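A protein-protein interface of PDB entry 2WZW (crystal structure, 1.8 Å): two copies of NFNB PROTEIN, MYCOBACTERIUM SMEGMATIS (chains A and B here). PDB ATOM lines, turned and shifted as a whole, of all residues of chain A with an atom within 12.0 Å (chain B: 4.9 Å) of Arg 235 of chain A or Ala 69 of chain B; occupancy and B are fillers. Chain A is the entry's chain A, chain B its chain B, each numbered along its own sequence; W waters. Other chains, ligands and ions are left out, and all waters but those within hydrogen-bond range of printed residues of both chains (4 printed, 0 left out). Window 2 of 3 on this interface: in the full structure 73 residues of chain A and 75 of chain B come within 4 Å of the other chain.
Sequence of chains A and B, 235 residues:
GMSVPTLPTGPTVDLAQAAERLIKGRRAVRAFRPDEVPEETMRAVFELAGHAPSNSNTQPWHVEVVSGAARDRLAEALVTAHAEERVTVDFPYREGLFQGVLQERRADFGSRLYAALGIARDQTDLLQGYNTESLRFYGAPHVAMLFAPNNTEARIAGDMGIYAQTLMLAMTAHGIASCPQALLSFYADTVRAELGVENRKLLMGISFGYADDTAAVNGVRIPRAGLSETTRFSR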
ATOM      1  N   THR A 231       9.156 -16.842 -26.067  1.00  0.00           N
ATOM      2  CA  THR A 231       9.664 -15.537 -26.497  1.00  0.00           C
ATOM      3  C   THR A 231       8.871 -14.386 -25.873  1.00  0.00           C
ATOM      4  O   THR A 231       7.646 -14.470 -25.721  1.00  0.00           O
ATOM      5  CB  THR A 231       9.627 -15.511 -28.047  1.00  0.00           C
ATOM      6  OG1 THR A 231      10.195 -16.730 -28.537  1.00  0.00           O
ATOM      7  CG2 THR A 231      10.344 -14.324 -28.652  1.00  0.00           C
ATOM      8  N   ARG A 232       9.572 -13.304 -25.529  1.00  0.00           N
ATOM      9  CA  ARG A 232       8.923 -12.131 -24.956  1.00  0.00           C
ATOM     10  C   ARG A 232       9.416 -10.911 -25.702  1.00  0.00           C
ATOM     11  O   ARG A 232      10.628 -10.705 -25.782  1.00  0.00           O
ATOM     12  CB  ARG A 232       9.228 -12.013 -23.450  1.00  0.00           C
ATOM     13  CG  ARG A 232       8.670 -10.698 -22.853  1.00  0.00           C
ATOM     14  CD  ARG A 232       8.917 -10.563 -21.373  1.00  0.00           C
ATOM     15  NE  ARG A 232       8.433  -9.265 -20.898  1.00  0.00           N
ATOM     16  CZ  ARG A 232       9.205  -8.295 -20.426  1.00  0.00           C
ATOM     17  NH1 ARG A 232      10.520  -8.467 -20.332  1.00  0.00           N
ATOM     18  NH2 ARG A 232       8.666  -7.158 -20.006  1.00  0.00           N
ATOM     19  N   PHE A 233       8.489 -10.106 -26.235  1.00  0.00           N
ATOM     20  CA  PHE A 233       8.834  -8.878 -26.966  1.00  0.00           C
ATOM     21  C   PHE A 233       8.592  -7.659 -26.088  1.00  0.00           C
ATOM     22  O   PHE A 233       7.514  -7.527 -25.503  1.00  0.00           O
ATOM     23  CB  PHE A 233       7.995  -8.749 -28.270  1.00  0.00           C
ATOM     24  CG  PHE A 233       8.241  -9.839 -29.290  1.00  0.00           C
ATOM     25  CD1 PHE A 233       7.529 -11.037 -29.242  1.00  0.00           C
ATOM     26  CD2 PHE A 233       9.209  -9.683 -30.280  1.00  0.00           C
ATOM     27  CE1 PHE A 233       7.786 -12.059 -30.160  1.00  0.00           C
ATOM     28  CE2 PHE A 233       9.462 -10.702 -31.203  1.00  0.00           C
ATOM     29  CZ  PHE A 233       8.741 -11.880 -31.147  1.00  0.00           C
ATOM     30  N   SER A 234       9.576  -6.760 -25.998  1.00  0.00           N
ATOM     31  CA  SER A 234       9.364  -5.529 -25.234  1.00  0.00           C
ATOM     32  C   SER A 234       9.886  -4.320 -25.996  1.00  0.00           C
ATOM     33  O   SER A 234      10.779  -4.440 -26.840  1.00  0.00           O
ATOM     34  CB  SER A 234       9.972  -5.621 -23.839  1.00  0.00           C
ATOM     35  OG  SER A 234      11.386  -5.580 -23.877  1.00  0.00           O
ATOM     36  N   ARG A 235       9.285  -3.159 -25.712  1.00  0.00           N
ATOM     37  CA  ARG A 235       9.625  -1.878 -26.306  1.00  0.00           C
ATOM     38  C   ARG A 235       9.371  -0.711 -25.345  1.00  0.00           C
ATOM     39  O   ARG A 235       9.879   0.396 -25.612  1.00  0.00           O
ATOM     40  CB  ARG A 235       9.012  -1.671 -27.707  1.00  0.00           C
ATOM     41  CG  ARG A 235       7.488  -1.621 -27.799  1.00  0.00           C
ATOM     42  CD  ARG A 235       7.024  -1.802 -29.244  1.00  0.00           C
ATOM     43  NE  ARG A 235       7.855  -1.032 -30.172  1.00  0.00           N
ATOM     44  CZ  ARG A 235       8.497  -1.532 -31.228  1.00  0.00           C
ATOM     45  NH1 ARG A 235       9.259  -0.749 -31.975  1.00  0.00           N
ATOM     46  NH2 ARG A 235       8.370  -2.816 -31.549  1.00  0.00           N
ATOM     47  OXT ARG A 235       8.760  -0.938 -24.274  1.00  0.00           O
ATOM     48  N   GLU B  36      13.334  -0.307 -38.642  1.00  0.00           N
ATOM     49  CA  GLU B  36      12.849  -1.463 -37.879  1.00  0.00           C
ATOM     50  C   GLU B  36      12.288  -2.558 -38.765  1.00  0.00           C
ATOM     51  O   GLU B  36      11.712  -2.286 -39.825  1.00  0.00           O
ATOM     52  CB  GLU B  36      11.750  -1.036 -36.893  1.00  0.00           C
ATOM     53  CG  GLU B  36      12.209  -0.096 -35.793  1.00  0.00           C
ATOM     54  CD  GLU B  36      11.126   0.135 -34.759  1.00  0.00           C
ATOM     55  OE1 GLU B  36      11.283  -0.364 -33.624  1.00  0.00           O
ATOM     56  OE2 GLU B  36      10.088   0.748 -35.100  1.00  0.00           O
ATOM     57  N   GLU B  39       6.605  -5.666 -37.218  1.00  0.00           N
ATOM     58  CA  GLU B  39       6.226  -6.599 -36.148  1.00  0.00           C
ATOM     59  C   GLU B  39       5.739  -7.962 -36.648  1.00  0.00           C
ATOM     60  O   GLU B  39       6.107  -8.972 -36.050  1.00  0.00           O
ATOM     61  CB  GLU B  39       5.201  -5.991 -35.185  1.00  0.00           C
ATOM     62  CG  GLU B  39       5.833  -5.208 -34.051  1.00  0.00           C
ATOM     63  CD  GLU B  39       4.822  -4.705 -33.041  1.00  0.00           C
ATOM     64  OE1 GLU B  39       4.317  -5.528 -32.243  1.00  0.00           O
ATOM     65  OE2 GLU B  39       4.527  -3.490 -33.056  1.00  0.00           O
ATOM     66  N   MET B  42       8.811 -10.044 -37.682  1.00  0.00           N
ATOM     67  CA  MET B  42       9.507 -10.538 -36.492  1.00  0.00           C
ATOM     68  C   MET B  42       8.740 -11.706 -35.885  1.00  0.00           C
ATOM     69  O   MET B  42       9.356 -12.703 -35.516  1.00  0.00           O
ATOM     70  CB  MET B  42       9.683  -9.440 -35.448  1.00  0.00           C
ATOM     71  CG  MET B  42      11.029  -8.789 -35.507  1.00  0.00           C
ATOM     72  SD  MET B  42      11.283  -7.604 -33.998  1.00  0.00           S
ATOM     73  CE  MET B  42       9.805  -6.399 -34.292  1.00  0.00           C
ATOM     74  N   SER B  67      13.192  -3.803 -28.489  1.00  0.00           N
ATOM     75  CA  SER B  67      13.069  -2.787 -29.542  1.00  0.00           C
ATOM     76  C   SER B  67      12.781  -1.410 -28.928  1.00  0.00           C
ATOM     77  O   SER B  67      12.556  -1.308 -27.716  1.00  0.00           O
ATOM     78  CB  SER B  67      11.919  -3.151 -30.488  1.00  0.00           C
ATOM     79  OG  SER B  67      12.047  -4.463 -31.010  1.00  0.00           O
ATOM     80  N   GLY B  68      12.760  -0.382 -29.782  1.00  0.00           N
ATOM     81  CA  GLY B  68      12.422   0.998 -29.427  1.00  0.00           C
ATOM     82  C   GLY B  68      13.107   1.569 -28.203  1.00  0.00           C
ATOM     83  O   GLY B  68      14.297   1.337 -28.003  1.00  0.00           O
ATOM     84  N   ALA B  69      12.362   2.357 -27.390  1.00  0.00           N
ATOM     85  CA  ALA B  69      12.896   3.001 -26.180  1.00  0.00           C
ATOM     86  C   ALA B  69      13.546   2.002 -25.202  1.00  0.00           C
ATOM     87  O   ALA B  69      14.591   2.324 -24.624  1.00  0.00           O
ATOM     88  CB  ALA B  69      11.806   3.810 -25.482  1.00  0.00           C
ATOM     89  N   ALA B  70      12.960   0.794 -25.041  1.00  0.00           N
ATOM     90  CA  ALA B  70      13.544  -0.241 -24.174  1.00  0.00           C
ATOM     91  C   ALA B  70      14.931  -0.652 -24.697  1.00  0.00           C
ATOM     92  O   ALA B  70      15.866  -0.812 -23.899  1.00  0.00           O
ATOM     93  CB  ALA B  70      12.630  -1.454 -24.117  1.00  0.00           C
ATOM     94  N   ARG B  71      15.072  -0.802 -26.040  1.00  0.00           N
ATOM     95  CA  ARG B  71      16.369  -1.149 -26.663  1.00  0.00           C
ATOM     96  C   ARG B  71      17.379  -0.003 -26.423  1.00  0.00           C
ATOM     97  O   ARG B  71      18.528  -0.269 -26.095  1.00  0.00           O
ATOM     98  CB  ARG B  71      16.181  -1.502 -28.161  1.00  0.00           C
ATOM     99  CG  ARG B  71      17.454  -1.495 -29.045  1.00  0.00           C
ATOM    100  CD  ARG B  71      17.577  -0.219 -29.885  1.00  0.00           C
ATOM    101  NE  ARG B  71      18.836  -0.250 -30.649  1.00  0.00           N
ATOM    102  CZ  ARG B  71      19.897   0.528 -30.427  1.00  0.00           C
ATOM    103  NH1 ARG B  71      21.004   0.375 -31.151  1.00  0.00           N
ATOM    104  NH2 ARG B  71      19.851   1.486 -29.503  1.00  0.00           N
ATOM    105  N   ASP B  72      16.944   1.261 -26.526  1.00  0.00           N
ATOM    106  CA  ASP B  72      17.830   2.400 -26.264  1.00  0.00           C
ATOM    107  C   ASP B  72      18.309   2.432 -24.810  1.00  0.00           C
ATOM    108  O   ASP B  72      19.501   2.636 -24.581  1.00  0.00           O
ATOM    109  CB  ASP B  72      17.152   3.728 -26.626  1.00  0.00           C
ATOM    110  CG  ASP B  72      16.848   3.881 -28.101  1.00  0.00           C
ATOM    111  OD1 ASP B  72      15.951   4.678 -28.436  1.00  0.00           O
ATOM    112  OD2 ASP B  72      17.501   3.191 -28.922  1.00  0.00           O
ATOM    113  N   ARG B  73      17.398   2.193 -23.828  1.00  0.00           N
ATOM    114  CA  ARG B  73      17.768   2.175 -22.402  1.00  0.00           C
ATOM    115  C   ARG B  73      18.716   1.035 -22.119  1.00  0.00           C
ATOM    116  O   ARG B  73      19.658   1.220 -21.356  1.00  0.00           O
ATOM    117  CB  ARG B  73      16.547   2.054 -21.474  1.00  0.00           C
ATOM    118  CG  ARG B  73      15.592   3.238 -21.534  1.00  0.00           C
ATOM    119  CD  ARG B  73      14.573   3.225 -20.397  1.00  0.00           C
ATOM    120  NE  ARG B  73      13.658   2.087 -20.464  1.00  0.00           N
ATOM    121  CZ  ARG B  73      12.558   2.033 -21.213  1.00  0.00           C
ATOM    122  NH1 ARG B  73      12.225   3.055 -21.991  1.00  0.00           N
ATOM    123  NH2 ARG B  73      11.795   0.950 -21.202  1.00  0.00           N
HETATM  124  O   HOH W   1       9.749   1.897 -23.286  1.00  0.00           O
HETATM  125  O   HOH W   2      10.548  -6.043 -29.362  1.00  0.00           O
HETATM  126  O   HOH W   3       9.417   2.321 -27.711  1.00  0.00           O
HETATM  127  O   HOH W   4       7.311   0.717 -34.372  1.00  0.00           O
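The backbone carbonyl oxygen (O) of Ser 234 of chain A is in hydrogen-bond range of the backbone NH (N) of Ser 67 of chain B, 3.0 Å away. The backbone NH (N) of Ala 70 of chain B sits at hydrogen-bond distance from the chain-end carboxylate (O) of Arg 235 of chain A, at 3.2 Å. NH1 of Arg 235 of chain A is in salt-bridge range of OE1 of Glu 36 of chain B (2.6 Å).
Among the printed residues, merely in contact across the chains: Arg 235 of chain A with Ser 67 of chain B (3.3 Å) and Arg 235 of chain A with Ala 69 of chain B (3.6 Å).
Thr 231 of chain A touches none of the printed residues of chain B. Arg 232 of chain A touches none of the printed residues of chain B. Of the printed residues of chain B, Ser 234 of chain A touches Ser 67. Arg 235 of chain A touches just these residues of chain B: Glu 36, Ser 67, Ala 69 and Ala 70. Printed residues of chain A within 4 Å of Glu 36 of chain B: Arg 235 (2.6 Å). Of the printed residues of chain A, Ser 67 of chain B touches Ser 234 (3.0 Å) and Arg 235 (3.3 Å). No residue of chain A comes within 4 Å of Gly 68 of chain B. No residue of chain A comes within 4 Å of Asp 72 of chain B. No residue of chain A comes within 4 Å of Arg 73 of chain B. The nearest printed residue of chain A that does not touch Ala 69 of chain B is Ser 234 of chain A (7.0 Å).
Of the 5 printed residues of chain A, 2 touch a printed residue of chain B. Hydrophobic or aromatic side chains of chain B that line the printed part of chain A: Ala 69 and Ala 70. Along chain B the printed residues that touch a printed residue of chain A span positions 36 to 70. Among the printed residues, Asp or Glu carboxylates within 4 Å of a Lys or Arg side-chain nitrogen of the other chain: Arg 235 of chain A with Glu 36 of chain B (2.6 Å).
No position is printed for both chains.
Water W2 bridges the side-chain hydroxyl of Ser 67 of chain B and the backbone carbonyl oxygen of Ser 234 of chain A. Water W1 bridges the chain-end carboxylate (O) of Arg 235 of chain A (2.8 Å) and the guanidinium group (NH1) of Arg 73 of chain B (3.0 Å). Water W4 lies within hydrogen-bond range of the side-chain carboxylate (OE2) of Glu 36 of chain B (2.9 Å) and the guanidinium group (NH1) of Arg 235 of chain A (3.4 Å). Water W3 bridges O of Arg 235 of chain A (2.9 Å) and N of Ala 69 of chain B (3.0 Å).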
